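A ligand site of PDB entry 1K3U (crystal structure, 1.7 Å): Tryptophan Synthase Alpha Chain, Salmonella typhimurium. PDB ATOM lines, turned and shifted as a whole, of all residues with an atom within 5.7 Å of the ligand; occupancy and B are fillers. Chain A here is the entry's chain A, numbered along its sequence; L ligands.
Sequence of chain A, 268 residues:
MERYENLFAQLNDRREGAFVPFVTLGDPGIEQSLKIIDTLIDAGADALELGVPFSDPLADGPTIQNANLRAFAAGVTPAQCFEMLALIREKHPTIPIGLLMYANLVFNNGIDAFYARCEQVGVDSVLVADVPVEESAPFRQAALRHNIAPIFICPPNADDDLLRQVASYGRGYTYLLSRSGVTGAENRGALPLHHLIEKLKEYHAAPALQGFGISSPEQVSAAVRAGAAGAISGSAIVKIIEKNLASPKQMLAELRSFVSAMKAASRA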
ATOM      1  N   PHE A  22       9.508 -14.774  23.239  1.00  0.00           N
ATOM      2  CA  PHE A  22      10.407 -15.909  22.933  1.00  0.00           C
ATOM      3  C   PHE A  22       9.862 -16.706  21.755  1.00  0.00           C
ATOM      4  O   PHE A  22       8.649 -16.914  21.624  1.00  0.00           O
ATOM      5  CB  PHE A  22      10.472 -16.863  24.123  1.00  0.00           C
ATOM      6  CG  PHE A  22      11.068 -18.225  23.780  1.00  0.00           C
ATOM      7  CD1 PHE A  22      10.262 -19.226  23.178  1.00  0.00           C
ATOM      8  CD2 PHE A  22      12.403 -18.454  23.910  1.00  0.00           C
ATOM      9  CE1 PHE A  22      10.848 -20.498  22.842  1.00  0.00           C
ATOM     10  CE2 PHE A  22      13.016 -19.668  23.567  1.00  0.00           C
ATOM     11  CZ  PHE A  22      12.281 -20.715  23.035  1.00  0.00           C
ATOM     12  N   GLU A  49      14.015 -13.241  23.174  1.00  0.00           N
ATOM     13  CA  GLU A  49      14.634 -14.422  23.786  1.00  0.00           C
ATOM     14  C   GLU A  49      14.463 -15.508  22.685  1.00  0.00           C
ATOM     15  O   GLU A  49      13.355 -15.712  22.152  1.00  0.00           O
ATOM     16  CB  GLU A  49      13.869 -14.813  25.016  1.00  0.00           C
ATOM     17  CG  GLU A  49      14.665 -15.826  25.750  1.00  0.00           C
ATOM     18  CD  GLU A  49      15.866 -15.184  26.430  1.00  0.00           C
ATOM     19  OE1 GLU A  49      15.978 -13.947  26.687  1.00  0.00           O
ATOM     20  OE2 GLU A  49      16.780 -15.942  26.627  1.00  0.00           O
ATOM     21  N   ALA A  59      13.429 -28.682  30.348  1.00  0.00           N
ATOM     22  CA  ALA A  59      12.688 -27.665  31.103  1.00  0.00           C
ATOM     23  C   ALA A  59      11.523 -27.084  30.318  1.00  0.00           C
ATOM     24  O   ALA A  59      10.917 -26.107  30.751  1.00  0.00           O
ATOM     25  CB  ALA A  59      13.596 -26.514  31.531  1.00  0.00           C
ATOM     26  N   ASP A  60      11.177 -27.710  29.215  1.00  0.00           N
ATOM     27  CA  ASP A  60      10.089 -27.163  28.406  1.00  0.00           C
ATOM     28  C   ASP A  60       8.867 -28.029  28.374  1.00  0.00           C
ATOM     29  O   ASP A  60       9.004 -29.264  28.244  1.00  0.00           O
ATOM     30  CB  ASP A  60      10.561 -27.039  26.955  1.00  0.00           C
ATOM     31  CG  ASP A  60      11.417 -25.767  26.762  1.00  0.00           C
ATOM     32  OD1 ASP A  60      10.820 -24.631  26.959  1.00  0.00           O
ATOM     33  OD2 ASP A  60      12.627 -25.836  26.511  1.00  0.00           O
ATOM     34  N   ILE A  64       6.695 -25.769  23.625  1.00  0.00           N
ATOM     35  CA  ILE A  64       8.051 -25.549  23.161  1.00  0.00           C
ATOM     36  C   ILE A  64       8.730 -26.895  22.763  1.00  0.00           C
ATOM     37  O   ILE A  64       9.567 -26.922  21.873  1.00  0.00           O
ATOM     38  CB  ILE A  64       8.813 -24.650  24.141  1.00  0.00           C
ATOM     39  CG1 ILE A  64       8.152 -23.213  24.104  1.00  0.00           C
ATOM     40  CG2 ILE A  64      10.291 -24.562  23.753  1.00  0.00           C
ATOM     41  CD1 ILE A  64       8.735 -22.324  25.181  1.00  0.00           C
ATOM     42  N   LEU A 100      18.256 -18.849  24.748  1.00  0.00           N
ATOM     43  CA  LEU A 100      17.804 -19.866  25.709  1.00  0.00           C
ATOM     44  C   LEU A 100      18.473 -21.155  25.232  1.00  0.00           C
ATOM     45  O   LEU A 100      18.171 -21.709  24.161  1.00  0.00           O
ATOM     46  CB  LEU A 100      16.276 -20.003  25.680  1.00  0.00           C
ATOM     47  CG  LEU A 100      15.706 -20.929  26.799  1.00  0.00           C
ATOM     48  CD1 LEU A 100      16.038 -22.390  26.473  1.00  0.00           C
ATOM     49  CD2 LEU A 100      16.181 -20.585  28.137  1.00  0.00           C
ATOM     50  N   TYR A 102      20.354 -25.129  26.204  1.00  0.00           N
ATOM     51  CA  TYR A 102      20.659 -26.205  27.141  1.00  0.00           C
ATOM     52  C   TYR A 102      22.171 -26.392  27.168  1.00  0.00           C
ATOM     53  O   TYR A 102      22.908 -26.172  26.217  1.00  0.00           O
ATOM     54  CB  TYR A 102      19.939 -27.505  26.681  1.00  0.00           C
ATOM     55  CG  TYR A 102      18.465 -27.368  27.087  1.00  0.00           C
ATOM     56  CD1 TYR A 102      17.989 -27.810  28.289  1.00  0.00           C
ATOM     57  CD2 TYR A 102      17.581 -26.767  26.230  1.00  0.00           C
ATOM     58  CE1 TYR A 102      16.636 -27.640  28.678  1.00  0.00           C
ATOM     59  CE2 TYR A 102      16.209 -26.619  26.569  1.00  0.00           C
ATOM     60  CZ  TYR A 102      15.744 -27.046  27.802  1.00  0.00           C
ATOM     61  OH  TYR A 102      14.375 -26.945  28.076  1.00  0.00           O
ATOM     62  N   LEU A 127      20.898 -17.673  28.686  1.00  0.00           N
ATOM     63  CA  LEU A 127      20.317 -18.361  29.843  1.00  0.00           C
ATOM     64  C   LEU A 127      20.506 -19.813  29.517  1.00  0.00           C
ATOM     65  O   LEU A 127      19.979 -20.319  28.530  1.00  0.00           O
ATOM     66  CB  LEU A 127      18.798 -17.992  29.926  1.00  0.00           C
ATOM     67  CG  LEU A 127      18.163 -18.315  31.266  1.00  0.00           C
ATOM     68  CD1 LEU A 127      16.628 -17.795  31.355  1.00  0.00           C
ATOM     69  CD2 LEU A 127      18.185 -19.824  31.530  1.00  0.00           C
ATOM     70  N   ALA A 129      19.429 -23.241  30.548  1.00  0.00           N
ATOM     71  CA  ALA A 129      18.292 -23.701  31.399  1.00  0.00           C
ATOM     72  C   ALA A 129      18.638 -24.746  32.503  1.00  0.00           C
ATOM     73  O   ALA A 129      17.989 -24.720  33.577  1.00  0.00           O
ATOM     74  CB  ALA A 129      17.168 -24.239  30.542  1.00  0.00           C
ATOM     75  N   ILE A 153      17.870 -17.836  36.553  1.00  0.00           N
ATOM     76  CA  ILE A 153      16.457 -17.964  36.935  1.00  0.00           C
ATOM     77  C   ILE A 153      16.421 -17.871  38.427  1.00  0.00           C
ATOM     78  O   ILE A 153      17.209 -18.471  39.119  1.00  0.00           O
ATOM     79  CB  ILE A 153      15.917 -19.341  36.491  1.00  0.00           C
ATOM     80  CG1 ILE A 153      15.674 -19.335  34.958  1.00  0.00           C
ATOM     81  CG2 ILE A 153      14.525 -19.640  37.136  1.00  0.00           C
ATOM     82  CD1 ILE A 153      15.285 -20.729  34.326  1.00  0.00           C
ATOM     83  N   TYR A 175      15.969 -13.525  35.409  1.00  0.00           N
ATOM     84  CA  TYR A 175      14.746 -14.184  34.969  1.00  0.00           C
ATOM     85  C   TYR A 175      13.929 -14.562  36.195  1.00  0.00           C
ATOM     86  O   TYR A 175      14.337 -15.444  36.988  1.00  0.00           O
ATOM     87  CB  TYR A 175      15.096 -15.475  34.185  1.00  0.00           C
ATOM     88  CG  TYR A 175      13.909 -16.038  33.393  1.00  0.00           C
ATOM     89  CD1 TYR A 175      12.866 -16.670  34.065  1.00  0.00           C
ATOM     90  CD2 TYR A 175      13.873 -15.964  32.032  1.00  0.00           C
ATOM     91  CE1 TYR A 175      11.762 -17.208  33.404  1.00  0.00           C
ATOM     92  CE2 TYR A 175      12.709 -16.551  31.362  1.00  0.00           C
ATOM     93  CZ  TYR A 175      11.710 -17.144  32.073  1.00  0.00           C
ATOM     94  OH  TYR A 175      10.567 -17.690  31.466  1.00  0.00           O
ATOM     95  N   ARG A 179       6.515 -19.662  38.660  1.00  0.00           N
ATOM     96  CA  ARG A 179       6.005 -20.896  39.301  1.00  0.00           C
ATOM     97  C   ARG A 179       6.971 -22.020  38.994  1.00  0.00           C
ATOM     98  O   ARG A 179       7.855 -21.897  38.121  1.00  0.00           O
ATOM     99  CB  ARG A 179       4.635 -21.301  38.689  1.00  0.00           C
ATOM    100  CG  ARG A 179       4.628 -21.327  37.103  1.00  0.00           C
ATOM    101  CD  ARG A 179       3.497 -22.121  36.455  1.00  0.00           C
ATOM    102  NE  ARG A 179       3.510 -22.102  35.002  1.00  0.00           N
ATOM    103  CZ  ARG A 179       4.295 -22.862  34.246  1.00  0.00           C
ATOM    104  NH1 ARG A 179       5.143 -23.727  34.822  1.00  0.00           N
ATOM    105  NH2 ARG A 179       4.223 -22.756  32.898  1.00  0.00           N
ATOM    106  N   VAL A 182       7.497 -26.484  34.193  1.00  0.00           N
ATOM    107  CA  VAL A 182       8.227 -26.208  32.944  1.00  0.00           C
ATOM    108  C   VAL A 182       7.493 -25.170  32.099  1.00  0.00           C
ATOM    109  O   VAL A 182       6.394 -24.723  32.455  1.00  0.00           O
ATOM    110  CB  VAL A 182       8.342 -27.509  32.081  1.00  0.00           C
ATOM    111  CG1 VAL A 182       9.167 -28.502  32.835  1.00  0.00           C
ATOM    112  CG2 VAL A 182       6.937 -28.075  31.742  1.00  0.00           C
ATOM    113  N   THR A 183       8.111 -24.726  30.992  1.00  0.00           N
ATOM    114  CA  THR A 183       7.490 -23.597  30.281  1.00  0.00           C
ATOM    115  C   THR A 183       6.057 -24.022  29.943  1.00  0.00           C
ATOM    116  O   THR A 183       5.801 -25.241  29.687  1.00  0.00           O
ATOM    117  CB  THR A 183       8.276 -23.280  28.983  1.00  0.00           C
ATOM    118  OG1 THR A 183       8.436 -24.463  28.180  1.00  0.00           O
ATOM    119  CG2 THR A 183       9.761 -22.835  29.365  1.00  0.00           C
ATOM    120  N   GLY A 184       5.124 -23.055  29.865  1.00  0.00           N
ATOM    121  CA  GLY A 184       3.791 -23.410  29.332  1.00  0.00           C
ATOM    122  C   GLY A 184       2.929 -22.151  29.485  1.00  0.00           C
ATOM    123  O   GLY A 184       3.158 -21.376  30.396  1.00  0.00           O
ATOM    124  N   ALA A 185       1.929 -22.005  28.630  1.00  0.00           N
ATOM    125  CA  ALA A 185       1.236 -20.758  28.585  1.00  0.00           C
ATOM    126  C   ALA A 185      -0.001 -20.777  29.482  1.00  0.00           C
ATOM    127  O   ALA A 185      -0.573 -19.725  29.838  1.00  0.00           O
ATOM    128  CB  ALA A 185       0.768 -20.514  27.082  1.00  0.00           C
ATOM    129  N   GLN A 210       9.638 -11.103  34.399  1.00  0.00           N
ATOM    130  CA  GLN A 210       8.863 -12.270  34.827  1.00  0.00           C
ATOM    131  C   GLN A 210       8.542 -13.216  33.690  1.00  0.00           C
ATOM    132  O   GLN A 210       8.092 -12.754  32.610  1.00  0.00           O
ATOM    133  CB  GLN A 210       7.555 -11.815  35.415  1.00  0.00           C
ATOM    134  CG  GLN A 210       6.820 -13.024  36.102  1.00  0.00           C
ATOM    135  CD  GLN A 210       5.603 -12.559  36.848  1.00  0.00           C
ATOM    136  OE1 GLN A 210       5.550 -11.409  37.277  1.00  0.00           O
ATOM    137  NE2 GLN A 210       4.639 -13.420  36.985  1.00  0.00           N
ATOM    138  N   GLY A 211       8.734 -14.520  33.900  1.00  0.00           N
ATOM    139  CA  GLY A 211       8.369 -15.469  32.832  1.00  0.00           C
ATOM    140  C   GLY A 211       7.809 -16.755  33.390  1.00  0.00           C
ATOM    141  O   GLY A 211       8.102 -17.057  34.567  1.00  0.00           O
ATOM    142  N   PHE A 212       7.110 -17.512  32.521  1.00  0.00           N
ATOM    143  CA  PHE A 212       6.370 -18.822  32.738  1.00  0.00           C
ATOM    144  C   PHE A 212       4.875 -18.482  32.918  1.00  0.00           C
ATOM    145  O   PHE A 212       4.494 -17.773  33.869  1.00  0.00           O
ATOM    146  CB  PHE A 212       6.785 -19.700  33.929  1.00  0.00           C
ATOM    147  CG  PHE A 212       7.973 -20.631  33.619  1.00  0.00           C
ATOM    148  CD1 PHE A 212       8.983 -20.194  32.823  1.00  0.00           C
ATOM    149  CD2 PHE A 212       8.017 -21.900  34.168  1.00  0.00           C
ATOM    150  CE1 PHE A 212      10.117 -21.019  32.557  1.00  0.00           C
ATOM    151  CE2 PHE A 212       9.124 -22.756  33.878  1.00  0.00           C
ATOM    152  CZ  PHE A 212      10.141 -22.307  33.080  1.00  0.00           C
ATOM    153  N   GLY A 213       4.062 -18.961  31.977  1.00  0.00           N
ATOM    154  CA  GLY A 213       2.619 -18.723  32.046  1.00  0.00           C
ATOM    155  C   GLY A 213       2.214 -17.287  31.650  1.00  0.00           C
ATOM    156  O   GLY A 213       1.024 -16.928  31.872  1.00  0.00           O
ATOM    157  N   ILE A 214       3.115 -16.452  31.038  1.00  0.00           N
ATOM    158  CA  ILE A 214       2.787 -15.041  30.757  1.00  0.00           C
ATOM    159  C   ILE A 214       2.066 -15.069  29.403  1.00  0.00           C
ATOM    160  O   ILE A 214       2.726 -15.167  28.335  1.00  0.00           O
ATOM    161  CB  ILE A 214       4.094 -14.197  30.624  1.00  0.00           C
ATOM    162  CG1 ILE A 214       4.760 -14.104  32.018  1.00  0.00           C
ATOM    163  CG2 ILE A 214       3.721 -12.770  30.151  1.00  0.00           C
ATOM    164  CD1 ILE A 214       3.919 -13.351  33.044  1.00  0.00           C
ATOM    165  N   SER A 215       0.729 -14.904  29.414  1.00  0.00           N
ATOM    166  CA  SER A 215      -0.022 -15.136  28.163  1.00  0.00           C
ATOM    167  C   SER A 215      -1.070 -14.063  27.807  1.00  0.00           C
ATOM    168  O   SER A 215      -1.778 -14.208  26.843  1.00  0.00           O
ATOM    169  CB  SER A 215      -0.759 -16.443  28.275  1.00  0.00           C
ATOM    170  OG  SER A 215       0.294 -17.445  28.363  1.00  0.00           O
ATOM    171  N   ILE A 232       8.375 -11.806  29.997  1.00  0.00           N
ATOM    172  CA  ILE A 232       8.718 -12.575  28.782  1.00  0.00           C
ATOM    173  C   ILE A 232       7.512 -13.529  28.465  1.00  0.00           C
ATOM    174  O   ILE A 232       6.952 -14.219  29.414  1.00  0.00           O
ATOM    175  CB  ILE A 232       9.986 -13.442  29.069  1.00  0.00           C
ATOM    176  CG1 ILE A 232      11.206 -12.530  29.211  1.00  0.00           C
ATOM    177  CG2 ILE A 232      10.170 -14.508  27.947  1.00  0.00           C
ATOM    178  CD1 ILE A 232      12.379 -13.297  29.955  1.00  0.00           C
ATOM    179  N   SER A 233       7.104 -13.609  27.195  1.00  0.00           N
ATOM    180  CA  SER A 233       6.058 -14.521  26.807  1.00  0.00           C
ATOM    181  C   SER A 233       6.628 -15.399  25.728  1.00  0.00           C
ATOM    182  O   SER A 233       7.085 -14.914  24.646  1.00  0.00           O
ATOM    183  CB  SER A 233       4.840 -13.751  26.249  1.00  0.00           C
ATOM    184  OG  SER A 233       3.852 -14.687  25.780  1.00  0.00           O
ATOM    185  N   GLY A 234       6.523 -16.709  25.940  1.00  0.00           N
ATOM    186  CA  GLY A 234       7.019 -17.605  24.934  1.00  0.00           C
ATOM    187  C   GLY A 234       6.010 -18.628  24.511  1.00  0.00           C
ATOM    188  O   GLY A 234       5.678 -18.616  23.350  1.00  0.00           O
ATOM    189  N   SER A 235       5.529 -19.471  25.419  1.00  0.00           N
ATOM    190  CA  SER A 235       4.638 -20.474  24.944  1.00  0.00           C
ATOM    191  C   SER A 235       3.456 -19.847  24.221  1.00  0.00           C
ATOM    192  O   SER A 235       2.943 -20.439  23.261  1.00  0.00           O
ATOM    193  CB  SER A 235       4.125 -21.304  26.136  1.00  0.00           C
ATOM    194  OG  SER A 235       5.257 -22.047  26.607  1.00  0.00           O
ATOM    195  N   ALA A 236       2.961 -18.709  24.707  1.00  0.00           N
ATOM    196  CA  ALA A 236       1.780 -18.110  24.060  1.00  0.00           C
ATOM    197  C   ALA A 236       2.102 -17.675  22.643  1.00  0.00           C
ATOM    198  O   ALA A 236       1.258 -17.795  21.746  1.00  0.00           O
ATOM    199  CB  ALA A 236       1.287 -16.860  24.837  1.00  0.00           C
HETATM  200  O1  LIG L   1       5.730 -17.093  30.372  1.00  0.00           O
HETATM  201  C1  LIG L   1       6.189 -17.408  29.156  1.00  0.00           C
HETATM  202  O2  LIG L   1       5.381 -17.611  28.147  1.00  0.00           O
HETATM  203  C2  LIG L   1       7.710 -17.464  28.931  1.00  0.00           C
HETATM  204  C3  LIG L   1       8.189 -18.937  29.179  1.00  0.00           C
HETATM  205  C4  LIG L   1       7.078 -19.947  28.904  1.00  0.00           C
HETATM  206  O3  LIG L   1       6.953 -20.455  27.662  1.00  0.00           O
HETATM  207  O4  LIG L   1       6.362 -20.343  29.866  1.00  0.00           O
HETATM  208  N1  LIG L   1       9.280 -19.255  28.246  1.00  0.00           N
HETATM  209  C5  LIG L   1      10.477 -18.536  28.214  1.00  0.00           C
HETATM  210  O5  LIG L   1      10.717 -17.639  29.010  1.00  0.00           O
HETATM  211  C6  LIG L   1      11.521 -18.985  27.186  1.00  0.00           C
HETATM  212  C7  LIG L   1      11.981 -20.398  27.521  1.00  0.00           C
HETATM  213  C8  LIG L   1      11.980 -21.508  26.645  1.00  0.00           C
HETATM  214  N2  LIG L   1      12.500 -22.580  27.350  1.00  0.00           N
HETATM  215  C9  LIG L   1      12.559 -20.800  28.746  1.00  0.00           C
HETATM  216  C10 LIG L   1      12.879 -20.098  29.908  1.00  0.00           C
HETATM  217  C11 LIG L   1      12.853 -22.158  28.628  1.00  0.00           C
HETATM  218  C12 LIG L   1      13.443 -22.836  29.705  1.00  0.00           C
HETATM  219  C13 LIG L   1      13.744 -22.156  30.863  1.00  0.00           C
HETATM  220  C14 LIG L   1      13.449 -20.793  30.959  1.00  0.00           C
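OH of Tyr 175 sits at hydrogen-bond distance from O5 of the ligand.
N of Ser 235 sits at hydrogen-bond distance from O3 of the ligand.
The side-chain hydroxyl (OG) of Ser 235 lies within hydrogen-bond range of an oxygen (O3) of the ligand (2.6 Å).
The backbone NH (N) of Phe 212 is in hydrogen-bond range of an oxygen (O1) of the ligand, 2.6 Å away.
The backbone NH (N) of Gly 234 lies within hydrogen-bond range of an oxygen (O2) of the ligand (2.6 Å).
A nitrogen (N2) of the ligand is in hydrogen-bond range of the side-chain carboxylate of Asp 60 (2.7 Å).
An oxygen (O1) of the ligand is in hydrogen-bond range of the backbone NH (N) of Ile 214 (2.8 Å).
An oxygen (O1) of the ligand is in hydrogen-bond range of the backbone NH of Gly 213 (3.0 Å).
N of Gly 184 is in hydrogen-bond range of O4 of the ligand (3.0 Å).
The side-chain hydroxyl (OG) of Ser 235 lies close to the backbone NH (N) of Gly 184 (3.4 Å).
OD1 of Asp 60 is in hydrogen-bond range of OG1 of Thr 183, at 2.7 Å.
The side-chain hydroxyl of Tyr 102 sits at hydrogen-bond distance from the side-chain carboxylate of Asp 60 (2.6 Å).
The backbone carbonyl oxygen (O) of Ile 214 is in hydrogen-bond range of the side-chain hydroxyl (OG) of Ser 233 (2.8 Å).
N of Gly 213 lies within hydrogen-bond range of O of Gly 184 (3.0 Å).
NH2 of Arg 179 sits at hydrogen-bond distance from O of Gly 184, 3.0 Å away.
The backbone NH (N) of Thr 183 sits at hydrogen-bond distance from the backbone carbonyl oxygen (O) of Ala 59 (3.1 Å).
The backbone NH (N) of Ile 232 sits at hydrogen-bond distance from the backbone carbonyl oxygen (O) of Gln 210 (2.8 Å).
O of Ile 232 sits close to O1 of the ligand (3.3 Å).
Merely in contact with the ligand: Thr 183 (3.2 Å), Phe 22 (3.4 Å), Ser 233 (3.4 Å), Ile 64 (3.6 Å), Leu 100 (3.6 Å), Gly 211 (3.7 Å) and Ile 153 (3.8 Å).
Hydrophobic or aromatic side chains that line the ligand: Phe 22, Ile 64, Leu 100, Ile 153, Tyr 175, Phe 212, Ile 214 and Ile 232.
Of the 27 residues printed, 16 come within 4 Å of the ligand.
The nearest printed residue that does not touch the ligand is Ala 129 (4.02 Å).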
